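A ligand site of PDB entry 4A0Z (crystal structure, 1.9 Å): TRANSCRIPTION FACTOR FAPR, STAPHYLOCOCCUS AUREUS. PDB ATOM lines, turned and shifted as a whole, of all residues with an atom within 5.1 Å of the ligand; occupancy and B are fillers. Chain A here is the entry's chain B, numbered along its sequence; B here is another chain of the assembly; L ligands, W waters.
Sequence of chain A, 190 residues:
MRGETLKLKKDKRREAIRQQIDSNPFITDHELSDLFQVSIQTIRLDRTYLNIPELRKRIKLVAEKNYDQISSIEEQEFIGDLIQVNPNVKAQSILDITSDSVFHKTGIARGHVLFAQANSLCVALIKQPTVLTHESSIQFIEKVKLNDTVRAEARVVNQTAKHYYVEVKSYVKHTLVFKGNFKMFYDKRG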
ATOM      1  N   ILE A  73      16.649 -37.431 -18.653  1.00  0.00           N
ATOM      2  CA  ILE A  73      17.819 -36.951 -17.912  1.00  0.00           C
ATOM      3  C   ILE A  73      18.536 -38.154 -17.313  1.00  0.00           C
ATOM      4  O   ILE A  73      17.914 -39.191 -17.094  1.00  0.00           O
ATOM      5  CB  ILE A  73      17.433 -35.901 -16.805  1.00  0.00           C
ATOM      6  CG1 ILE A  73      18.680 -35.212 -16.230  1.00  0.00           C
ATOM      7  CG2 ILE A  73      16.601 -36.524 -15.705  1.00  0.00           C
ATOM      8  CD1 ILE A  73      18.376 -33.945 -15.401  1.00  0.00           C
ATOM      9  N   ASN A 119      14.109 -28.042 -10.754  1.00  0.00           N
ATOM     10  CA  ASN A 119      14.152 -28.070 -12.217  1.00  0.00           C
ATOM     11  C   ASN A 119      14.475 -29.482 -12.754  1.00  0.00           C
ATOM     12  O   ASN A 119      13.751 -30.027 -13.604  1.00  0.00           O
ATOM     13  CB  ASN A 119      15.185 -27.032 -12.704  1.00  0.00           C
ATOM     14  CG  ASN A 119      14.964 -26.631 -14.145  1.00  0.00           C
ATOM     15  OD1 ASN A 119      13.811 -26.586 -14.612  1.00  0.00           O
ATOM     16  ND2 ASN A 119      16.058 -26.332 -14.856  1.00  0.00           N
ATOM     17  N   SER A 120      15.533 -30.110 -12.232  1.00  0.00           N
ATOM     18  CA  SER A 120      15.895 -31.508 -12.581  1.00  0.00           C
ATOM     19  C   SER A 120      14.754 -32.471 -12.338  1.00  0.00           C
ATOM     20  O   SER A 120      14.556 -33.417 -13.103  1.00  0.00           O
ATOM     21  CB  SER A 120      17.056 -32.032 -11.723  1.00  0.00           C
ATOM     22  OG  SER A 120      18.223 -31.266 -11.942  1.00  0.00           O
ATOM     23  N   VAL A 123      12.150 -32.239 -15.099  1.00  0.00           N
ATOM     24  CA  VAL A 123      12.655 -32.908 -16.286  1.00  0.00           C
ATOM     25  C   VAL A 123      12.469 -34.420 -16.159  1.00  0.00           C
ATOM     26  O   VAL A 123      11.903 -35.056 -17.046  1.00  0.00           O
ATOM     27  CB  VAL A 123      14.151 -32.588 -16.556  1.00  0.00           C
ATOM     28  CG1 VAL A 123      14.682 -33.441 -17.735  1.00  0.00           C
ATOM     29  CG2 VAL A 123      14.330 -31.131 -16.817  1.00  0.00           C
ATOM     30  N   THR A 130      12.652 -35.387 -25.630  1.00  0.00           N
ATOM     31  CA  THR A 130      13.075 -33.999 -25.438  1.00  0.00           C
ATOM     32  C   THR A 130      12.176 -33.295 -24.429  1.00  0.00           C
ATOM     33  O   THR A 130      10.946 -33.279 -24.588  1.00  0.00           O
ATOM     34  CB  THR A 130      13.061 -33.207 -26.778  1.00  0.00           C
ATOM     35  OG1 THR A 130      13.980 -33.811 -27.685  1.00  0.00           O
ATOM     36  CG2 THR A 130      13.472 -31.742 -26.554  1.00  0.00           C
ATOM     37  N   VAL A 131      12.788 -32.728 -23.391  1.00  0.00           N
ATOM     38  CA  VAL A 131      12.092 -32.003 -22.337  1.00  0.00           C
ATOM     39  C   VAL A 131      12.956 -30.824 -21.994  1.00  0.00           C
ATOM     40  O   VAL A 131      14.119 -30.995 -21.592  1.00  0.00           O
ATOM     41  CB  VAL A 131      11.881 -32.855 -21.045  1.00  0.00           C
ATOM     42  CG1 VAL A 131      11.219 -32.031 -19.920  1.00  0.00           C
ATOM     43  CG2 VAL A 131      11.063 -34.089 -21.349  1.00  0.00           C
ATOM     44  N   LEU A 132      12.417 -29.614 -22.143  1.00  0.00           N
ATOM     45  CA  LEU A 132      13.172 -28.408 -21.795  1.00  0.00           C
ATOM     46  C   LEU A 132      12.342 -27.427 -20.970  1.00  0.00           C
ATOM     47  O   LEU A 132      11.177 -27.183 -21.268  1.00  0.00           O
ATOM     48  CB  LEU A 132      13.649 -27.723 -23.069  1.00  0.00           C
ATOM     49  CG  LEU A 132      14.479 -28.536 -24.063  1.00  0.00           C
ATOM     50  CD1 LEU A 132      14.488 -27.870 -25.464  1.00  0.00           C
ATOM     51  CD2 LEU A 132      15.898 -28.701 -23.520  1.00  0.00           C
ATOM     52  N   THR A 133      12.947 -26.836 -19.935  1.00  0.00           N
ATOM     53  CA  THR A 133      12.207 -25.843 -19.163  1.00  0.00           C
ATOM     54  C   THR A 133      11.952 -24.611 -20.043  1.00  0.00           C
ATOM     55  O   THR A 133      12.872 -24.040 -20.617  1.00  0.00           O
ATOM     56  CB  THR A 133      12.936 -25.460 -17.870  1.00  0.00           C
ATOM     57  OG1 THR A 133      13.265 -26.667 -17.158  1.00  0.00           O
ATOM     58  CG2 THR A 133      12.018 -24.565 -16.979  1.00  0.00           C
ATOM     59  N   HIS A 134      10.687 -24.238 -20.145  1.00  0.00           N
ATOM     60  CA  HIS A 134      10.344 -23.062 -20.958  1.00  0.00           C
ATOM     61  C   HIS A 134      10.141 -21.846 -20.077  1.00  0.00           C
ATOM     62  O   HIS A 134      10.675 -20.773 -20.361  1.00  0.00           O
ATOM     63  CB  HIS A 134       9.087 -23.321 -21.820  1.00  0.00           C
ATOM     64  CG  HIS A 134       9.062 -22.511 -23.074  1.00  0.00           C
ATOM     65  ND1 HIS A 134       8.196 -22.792 -24.117  1.00  0.00           N
ATOM     66  CD2 HIS A 134       9.807 -21.454 -23.469  1.00  0.00           C
ATOM     67  CE1 HIS A 134       8.405 -21.926 -25.098  1.00  0.00           C
ATOM     68  NE2 HIS A 134       9.374 -21.099 -24.723  1.00  0.00           N
ATOM     69  N   LYS A 162       2.133 -29.139 -26.371  1.00  0.00           N
ATOM     70  CA  LYS A 162       3.523 -28.651 -26.371  1.00  0.00           C
ATOM     71  C   LYS A 162       4.203 -28.568 -25.002  1.00  0.00           C
ATOM     72  O   LYS A 162       5.434 -28.584 -24.901  1.00  0.00           O
ATOM     73  CB  LYS A 162       3.592 -27.304 -27.127  1.00  0.00           C
ATOM     74  CG  LYS A 162       4.936 -26.595 -27.101  1.00  0.00           C
ATOM     75  CD  LYS A 162       4.993 -25.492 -28.174  1.00  0.00           C
ATOM     76  CE  LYS A 162       6.310 -24.707 -28.136  1.00  0.00           C
ATOM     77  NZ  LYS A 162       6.533 -24.024 -29.443  1.00  0.00           N
ATOM     78  N   PHE A 185       8.448 -27.536 -21.897  1.00  0.00           N
ATOM     79  CA  PHE A 185       8.326 -27.921 -23.299  1.00  0.00           C
ATOM     80  C   PHE A 185       8.663 -29.394 -23.471  1.00  0.00           C
ATOM     81  O   PHE A 185       9.585 -29.918 -22.838  1.00  0.00           O
ATOM     82  CB  PHE A 185       9.260 -27.059 -24.189  1.00  0.00           C
ATOM     83  CG  PHE A 185       9.388 -27.552 -25.611  1.00  0.00           C
ATOM     84  CD1 PHE A 185       8.502 -27.140 -26.586  1.00  0.00           C
ATOM     85  CD2 PHE A 185      10.428 -28.414 -25.967  1.00  0.00           C
ATOM     86  CE1 PHE A 185       8.619 -27.600 -27.903  1.00  0.00           C
ATOM     87  CE2 PHE A 185      10.570 -28.861 -27.268  1.00  0.00           C
ATOM     88  CZ  PHE A 185       9.665 -28.455 -28.254  1.00  0.00           C
ATOM     89  N   ASP A 187       8.971 -32.671 -26.628  1.00  0.00           N
ATOM     90  CA  ASP A 187       8.899 -33.121 -28.004  1.00  0.00           C
ATOM     91  C   ASP A 187       9.203 -34.601 -28.076  1.00  0.00           C
ATOM     92  O   ASP A 187       9.997 -35.120 -27.292  1.00  0.00           O
ATOM     93  CB  ASP A 187       9.900 -32.349 -28.874  1.00  0.00           C
ATOM     94  CG  ASP A 187       9.520 -32.360 -30.347  1.00  0.00           C
ATOM     95  OD1 ASP A 187       9.639 -33.414 -31.011  1.00  0.00           O
ATOM     96  OD2 ASP A 187       9.089 -31.300 -30.827  1.00  0.00           O
ATOM     97  N   ARG A 189      10.423 -36.126 -30.768  1.00  0.00           N
ATOM     98  CA  ARG A 189      11.130 -36.349 -32.031  1.00  0.00           C
ATOM     99  C   ARG A 189      12.595 -35.928 -31.914  1.00  0.00           C
ATOM    100  O   ARG A 189      13.234 -36.198 -30.889  1.00  0.00           O
ATOM    101  CB  ARG A 189      10.381 -35.611 -33.152  1.00  0.00           C
ATOM    102  CG  ARG A 189      11.220 -35.072 -34.289  1.00  0.00           C
ATOM    103  CD  ARG A 189      10.480 -33.940 -35.025  1.00  0.00           C
ATOM    104  NE  ARG A 189      10.776 -32.608 -34.475  1.00  0.00           N
ATOM    105  CZ  ARG A 189       9.894 -31.824 -33.868  1.00  0.00           C
ATOM    106  NH1 ARG A 189       8.637 -32.189 -33.722  1.00  0.00           N
ATOM    107  NH2 ARG A 189      10.280 -30.631 -33.417  1.00  0.00           N
ATOM    108  N   PHE B 103      24.041 -30.134 -20.587  1.00  0.00           N
ATOM    109  CA  PHE B 103      23.727 -31.533 -20.882  1.00  0.00           C
ATOM    110  C   PHE B 103      24.752 -32.031 -21.897  1.00  0.00           C
ATOM    111  O   PHE B 103      24.833 -31.525 -23.026  1.00  0.00           O
ATOM    112  CB  PHE B 103      22.318 -31.677 -21.457  1.00  0.00           C
ATOM    113  CG  PHE B 103      21.227 -31.409 -20.470  1.00  0.00           C
ATOM    114  CD1 PHE B 103      20.927 -32.334 -19.471  1.00  0.00           C
ATOM    115  CD2 PHE B 103      20.466 -30.256 -20.559  1.00  0.00           C
ATOM    116  CE1 PHE B 103      19.895 -32.103 -18.559  1.00  0.00           C
ATOM    117  CE2 PHE B 103      19.425 -30.006 -19.641  1.00  0.00           C
ATOM    118  CZ  PHE B 103      19.143 -30.941 -18.651  1.00  0.00           C
ATOM    119  N   ILE B 108      23.308 -28.402 -24.551  1.00  0.00           N
ATOM    120  CA  ILE B 108      22.415 -27.355 -24.026  1.00  0.00           C
ATOM    121  C   ILE B 108      22.717 -26.991 -22.561  1.00  0.00           C
ATOM    122  O   ILE B 108      22.801 -27.871 -21.703  1.00  0.00           O
ATOM    123  CB  ILE B 108      20.909 -27.779 -24.172  1.00  0.00           C
ATOM    124  CG1 ILE B 108      20.529 -27.973 -25.648  1.00  0.00           C
ATOM    125  CG2 ILE B 108      19.986 -26.767 -23.476  1.00  0.00           C
ATOM    126  CD1 ILE B 108      19.237 -28.806 -25.862  1.00  0.00           C
ATOM    127  N   ALA B 109      22.855 -25.704 -22.284  1.00  0.00           N
ATOM    128  CA  ALA B 109      23.125 -25.240 -20.927  1.00  0.00           C
ATOM    129  C   ALA B 109      21.940 -25.506 -19.967  1.00  0.00           C
ATOM    130  O   ALA B 109      20.787 -25.279 -20.315  1.00  0.00           O
ATOM    131  CB  ALA B 109      23.505 -23.764 -20.911  1.00  0.00           C
ATOM    132  N   ARG B 110      22.287 -25.976 -18.766  1.00  0.00           N
ATOM    133  CA  ARG B 110      21.325 -26.244 -17.717  1.00  0.00           C
ATOM    134  C   ARG B 110      20.605 -24.968 -17.333  1.00  0.00           C
ATOM    135  O   ARG B 110      21.225 -23.903 -17.222  1.00  0.00           O
ATOM    136  CB  ARG B 110      22.035 -26.814 -16.474  1.00  0.00           C
ATOM    137  CG  ARG B 110      22.848 -28.090 -16.727  1.00  0.00           C
ATOM    138  CD  ARG B 110      21.957 -29.224 -17.249  1.00  0.00           C
ATOM    139  NE  ARG B 110      20.821 -29.541 -16.374  1.00  0.00           N
ATOM    140  CZ  ARG B 110      20.894 -30.357 -15.315  1.00  0.00           C
ATOM    141  NH1 ARG B 110      22.049 -30.917 -14.980  1.00  0.00           N
ATOM    142  NH2 ARG B 110      19.809 -30.629 -14.587  1.00  0.00           N
ATOM    143  N   GLY B 111      19.289 -25.081 -17.070  1.00  0.00           N
ATOM    144  CA  GLY B 111      18.523 -23.904 -16.668  1.00  0.00           C
ATOM    145  C   GLY B 111      19.029 -23.274 -15.386  1.00  0.00           C
ATOM    146  O   GLY B 111      19.010 -22.045 -15.234  1.00  0.00           O
ATOM    147  N   HIS B 112      19.503 -24.087 -14.433  1.00  0.00           N
ATOM    148  CA  HIS B 112      19.983 -23.487 -13.199  1.00  0.00           C
ATOM    149  C   HIS B 112      21.236 -22.669 -13.382  1.00  0.00           C
ATOM    150  O   HIS B 112      21.538 -21.847 -12.538  1.00  0.00           O
ATOM    151  CB  HIS B 112      20.224 -24.521 -12.090  1.00  0.00           C
ATOM    152  CG  HIS B 112      21.342 -25.476 -12.376  1.00  0.00           C
ATOM    153  ND1 HIS B 112      21.122 -26.752 -12.846  1.00  0.00           N
ATOM    154  CD2 HIS B 112      22.683 -25.333 -12.263  1.00  0.00           C
ATOM    155  CE1 HIS B 112      22.285 -27.364 -12.990  1.00  0.00           C
ATOM    156  NE2 HIS B 112      23.255 -26.521 -12.654  1.00  0.00           N
ATOM    157  N   PHE B 140      13.038 -19.027 -20.501  1.00  0.00           N
ATOM    158  CA  PHE B 140      14.128 -19.541 -21.298  1.00  0.00           C
ATOM    159  C   PHE B 140      13.709 -19.429 -22.765  1.00  0.00           C
ATOM    160  O   PHE B 140      12.991 -20.272 -23.293  1.00  0.00           O
ATOM    161  CB  PHE B 140      14.428 -20.995 -20.901  1.00  0.00           C
ATOM    162  CG  PHE B 140      14.848 -21.152 -19.455  1.00  0.00           C
ATOM    163  CD1 PHE B 140      16.163 -20.918 -19.063  1.00  0.00           C
ATOM    164  CD2 PHE B 140      13.920 -21.565 -18.494  1.00  0.00           C
ATOM    165  CE1 PHE B 140      16.570 -21.120 -17.760  1.00  0.00           C
ATOM    166  CE2 PHE B 140      14.313 -21.752 -17.155  1.00  0.00           C
ATOM    167  CZ  PHE B 140      15.652 -21.506 -16.783  1.00  0.00           C
ATOM    168  N   ILE B 141      14.151 -18.371 -23.410  1.00  0.00           N
ATOM    169  CA  ILE B 141      13.623 -17.988 -24.712  1.00  0.00           C
ATOM    170  C   ILE B 141      14.291 -18.760 -25.870  1.00  0.00           C
ATOM    171  O   ILE B 141      13.619 -19.199 -26.790  1.00  0.00           O
ATOM    172  CB  ILE B 141      13.729 -16.447 -24.905  1.00  0.00           C
ATOM    173  CG1 ILE B 141      12.931 -15.733 -23.804  1.00  0.00           C
ATOM    174  CG2 ILE B 141      13.311 -15.998 -26.309  1.00  0.00           C
ATOM    175  CD1 ILE B 141      13.444 -14.364 -23.514  1.00  0.00           C
ATOM    176  N   GLU B 142      15.620 -18.892 -25.806  1.00  0.00           N
ATOM    177  CA  GLU B 142      16.410 -19.644 -26.776  1.00  0.00           C
ATOM    178  C   GLU B 142      17.404 -20.528 -26.023  1.00  0.00           C
ATOM    179  O   GLU B 142      17.848 -20.184 -24.933  1.00  0.00           O
ATOM    180  CB  GLU B 142      17.182 -18.724 -27.717  1.00  0.00           C
ATOM    181  CG  GLU B 142      16.407 -17.542 -28.267  1.00  0.00           C
ATOM    182  CD  GLU B 142      15.767 -17.838 -29.589  1.00  0.00           C
ATOM    183  OE1 GLU B 142      14.919 -18.739 -29.621  1.00  0.00           O
ATOM    184  OE2 GLU B 142      16.116 -17.161 -30.602  1.00  0.00           O
ATOM    185  N   LYS B 143      17.750 -21.655 -26.629  1.00  0.00           N
ATOM    186  CA  LYS B 143      18.757 -22.554 -26.065  1.00  0.00           C
ATOM    187  C   LYS B 143      20.107 -21.852 -26.017  1.00  0.00           C
ATOM    188  O   LYS B 143      20.535 -21.253 -26.999  1.00  0.00           O
ATOM    189  CB  LYS B 143      18.893 -23.801 -26.930  1.00  0.00           C
ATOM    190  CG  LYS B 143      17.771 -24.805 -26.791  1.00  0.00           C
ATOM    191  CD  LYS B 143      17.948 -25.882 -27.853  1.00  0.00           C
ATOM    192  CE  LYS B 143      16.640 -26.581 -28.177  1.00  0.00           C
ATOM    193  NZ  LYS B 143      15.648 -25.695 -28.858  1.00  0.00           N
ATOM    194  N   VAL B 144      20.760 -21.940 -24.868  1.00  0.00           N
ATOM    195  CA  VAL B 144      22.152 -21.540 -24.743  1.00  0.00           C
ATOM    196  C   VAL B 144      22.988 -22.789 -24.939  1.00  0.00           C
ATOM    197  O   VAL B 144      22.615 -23.875 -24.467  1.00  0.00           O
ATOM    198  CB  VAL B 144      22.434 -20.879 -23.372  1.00  0.00           C
ATOM    199  CG1 VAL B 144      23.955 -20.607 -23.208  1.00  0.00           C
ATOM    200  CG2 VAL B 144      21.637 -19.616 -23.236  1.00  0.00           C
HETATM  201  C1  LIG L   1      12.985 -31.221 -32.519  1.00  0.00           C
HETATM  202  N1  LIG L   1      13.597 -31.065 -31.320  1.00  0.00           N
HETATM  203  C2  LIG L   1      14.564 -31.995 -31.209  1.00  0.00           C
HETATM  204  C3  LIG L   1      14.518 -32.766 -32.465  1.00  0.00           C
HETATM  205  N2  LIG L   1      13.537 -32.249 -33.219  1.00  0.00           N
HETATM  206  N3  LIG L   1      15.491 -32.315 -30.256  1.00  0.00           N
HETATM  207  C4  LIG L   1      16.356 -33.333 -30.462  1.00  0.00           C
HETATM  208  N4  LIG L   1      16.370 -34.095 -31.584  1.00  0.00           N
HETATM  209  C5  LIG L   1      15.501 -33.876 -32.608  1.00  0.00           C
HETATM  210  N5  LIG L   1      15.523 -34.644 -33.730  1.00  0.00           N
HETATM  211  C6  LIG L   1      13.270 -30.038 -30.305  1.00  0.00           C
HETATM  212  C7  LIG L   1      14.325 -28.944 -30.406  1.00  0.00           C
HETATM  213  O1  LIG L   1      14.511 -28.333 -29.120  1.00  0.00           O
HETATM  214  C8  LIG L   1      13.676 -27.968 -31.353  1.00  0.00           C
HETATM  215  O2  LIG L   1      14.200 -26.648 -31.280  1.00  0.00           O
HETATM  216  C9  LIG L   1      12.224 -28.024 -30.919  1.00  0.00           C
HETATM  217  O3  LIG L   1      12.003 -29.408 -30.606  1.00  0.00           O
HETATM  218  C10 LIG L   1      11.283 -27.522 -32.004  1.00  0.00           C
HETATM  219  O4  LIG L   1       9.953 -27.560 -31.513  1.00  0.00           O
HETATM  220  P1  LIG L   1       8.960 -26.308 -31.591  1.00  0.00           P
HETATM  221  O5  LIG L   1       7.708 -26.697 -30.868  1.00  0.00           O
HETATM  222  O6  LIG L   1       8.937 -25.801 -33.032  1.00  0.00           O
HETATM  223  O7  LIG L   1       9.774 -25.233 -30.706  1.00  0.00           O
HETATM  224  P2  LIG L   1       9.909 -23.628 -30.798  1.00  0.00           P
HETATM  225  O8  LIG L   1       8.585 -22.971 -30.499  1.00  0.00           O
HETATM  226  O9  LIG L   1      10.756 -23.231 -31.998  1.00  0.00           O
HETATM  227  O10 LIG L   1      10.835 -23.369 -29.507  1.00  0.00           O
HETATM  228  C11 LIG L   1      10.366 -23.818 -28.226  1.00  0.00           C
HETATM  229  C12 LIG L   1      11.561 -24.210 -27.375  1.00  0.00           C
HETATM  230  C13 LIG L   1      12.617 -23.084 -27.459  1.00  0.00           C
HETATM  231  C14 LIG L   1      11.065 -24.445 -25.946  1.00  0.00           C
HETATM  232  C15 LIG L   1      12.106 -25.490 -28.007  1.00  0.00           C
HETATM  233  O11 LIG L   1      11.994 -21.835 -27.166  1.00  0.00           O
HETATM  234  C16 LIG L   1      13.814 -23.230 -26.552  1.00  0.00           C
HETATM  235  O12 LIG L   1      14.671 -24.059 -26.790  1.00  0.00           O
HETATM  236  N6  LIG L   1      13.889 -22.381 -25.517  1.00  0.00           N
HETATM  237  C17 LIG L   1      14.998 -22.537 -24.579  1.00  0.00           C
HETATM  238  C18 LIG L   1      14.766 -23.720 -23.661  1.00  0.00           C
HETATM  239  C19 LIG L   1      15.918 -23.979 -22.718  1.00  0.00           C
HETATM  240  O13 LIG L   1      17.083 -23.888 -23.098  1.00  0.00           O
HETATM  241  N7  LIG L   1      15.578 -24.339 -21.473  1.00  0.00           N
HETATM  242  C20 LIG L   1      16.535 -24.411 -20.381  1.00  0.00           C
HETATM  243  C21 LIG L   1      17.501 -25.587 -20.443  1.00  0.00           C
HETATM  244  S1  LIG L   1      16.686 -27.090 -20.037  1.00  0.00           S
HETATM  245  P3  LIG L   1      14.862 -25.930 -32.582  1.00  0.00           P
HETATM  246  O14 LIG L   1      16.064 -26.804 -32.808  1.00  0.00           O
HETATM  247  O15 LIG L   1      13.823 -26.045 -33.664  1.00  0.00           O
HETATM  248  O16 LIG L   1      15.045 -24.530 -32.035  1.00  0.00           O
HETATM  249  C22 LIG L   1      16.454 -27.036 -18.368  1.00  0.00           C
HETATM  250  C23 LIG L   1      16.299 -28.313 -17.568  1.00  0.00           C
HETATM  251  C24 LIG L   1      17.515 -28.651 -16.730  1.00  0.00           C
HETATM  252  O17 LIG L   1      16.406 -25.948 -17.801  1.00  0.00           O
HETATM  253  O18 LIG L   1      18.532 -27.937 -16.764  1.00  0.00           O
HETATM  254  O19 LIG L   1      17.474 -29.675 -16.001  1.00  0.00           O
HETATM  255  O   HOH W   1       7.190 -29.126 -31.206  1.00  0.00           O
HETATM  256  O   HOH W   2      18.762 -26.909 -14.281  1.00  0.00           O
HETATM  257  O   HOH W   3      19.791 -23.498 -22.378  1.00  0.00           O
HETATM  258  O   HOH W   4      10.698 -19.207 -26.340  1.00  0.00           O
HETATM  259  O   HOH W   5      16.354 -30.161 -28.228  1.00  0.00           O
HETATM  260  O   HOH W   6      13.492 -22.383 -31.641  1.00  0.00           O
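The side-chain hydroxyl of Thr 130 sits at hydrogen-bond distance from a nitrogen (N3) of the ligand, 3.3 Å away. A nitrogen (N2) of the ligand is in hydrogen-bond range of the guanidinium group (NE) of Arg 189, 3.1 Å away. The backbone carbonyl oxygen (O) of Thr 133 lies within hydrogen-bond range of a nitrogen (N7) of the ligand (2.9 Å). The side-chain amino group (NZ) of Lys 143 of chain B is in salt-bridge range of an oxygen (O16) of the ligand (3.4 Å). O17 of the ligand sits at hydrogen-bond distance from OG1 of Thr 133, at 3.3 Å. The backbone NH (N) of Thr 133 lies close to a sulfur (S1) of the ligand (3.7 Å). O of Ile 141 of chain B sits at hydrogen-bond distance from O11 of the ligand (3.1 Å). The backbone carbonyl oxygen (O) of Phe 140 of chain B lies within hydrogen-bond range of a nitrogen (N6) of the ligand (3.2 Å). The backbone NH (N) of Gly 111 of chain B is in hydrogen-bond range of an oxygen (O18) of the ligand (3.0 Å). The side-chain amide nitrogen of Asn 119 is in hydrogen-bond range of an oxygen (O17) of the ligand (3.0 Å). NZ of Lys 162 lies within salt-bridge range of O8 of the ligand, 2.5 Å away. An oxygen (O18) of the ligand lies within salt-bridge range of the guanidinium group (NE) of Arg 110 of chain B (2.8 Å).
The backbone carbonyl oxygen of Thr 130 sits at hydrogen-bond distance from the backbone NH of Asp 187. OG1 of Thr 133 is in hydrogen-bond range of OD1 of Asn 119 (2.6 Å). The backbone carbonyl oxygen (O) of Leu 132 is in hydrogen-bond range of the backbone NH (N) of Phe 185, 2.8 Å away. O of Ile 108 of chain B lies within hydrogen-bond range of N of Phe 103 of chain B. NH2 of Arg 110 of chain B sits at hydrogen-bond distance from OG of Ser 120, at 3.1 Å. N of Phe 140 of chain B is in hydrogen-bond range of O of His 134 (2.9 Å). NH2 of Arg 189 lies within salt-bridge range of OD2 of Asp 187, at 2.9 Å.
O3 of the ligand sits close to OD2 of Asp 187 (3.5 Å). Residues that only touch the ligand: Phe 185 (3.2 Å), Ala 109 of chain B (3.3 Å), Phe 103 of chain B (3.4 Å), Glu 142 of chain B (3.5 Å), Val 123 (3.5 Å), His 134 (3.7 Å) and Leu 132 (3.7 Å). Within 4 Å of the ligand: Asn 119, Val 123, Thr 130, Leu 132, Thr 133, His 134, Lys 162, Phe 185, Asp 187, Arg 189, Phe 103 of chain B, Ala 109 of chain B, Arg 110 of chain B, Gly 111 of chain B, Phe 140 of chain B, Ile 141 of chain B, Glu 142 of chain B and Lys 143 of chain B.
Water W1 lies within hydrogen-bond range of O5 of the ligand (2.5 Å) and OD2 of Asp 187 (2.9 Å). Water W2 lies within hydrogen-bond range of an oxygen (O18) of the ligand (2.7 Å), a ring nitrogen (ND1) of His 112 of chain B (2.8 Å), the side-chain amide nitrogen (ND2) of Asn 119 (2.8 Å) and the backbone NH (N) of Gly 111 of chain B (3.4 Å). Water W3 bridges an oxygen (O13) of the ligand and the backbone carbonyl oxygen (O) of Ala 109 of chain B. Water W4 lies within hydrogen-bond range of a ring nitrogen (NE2) of His 134 (2.8 Å), the backbone carbonyl oxygen of Ile 141 of chain B (3.0 Å) and an oxygen (O11) of the ligand (3.0 Å).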
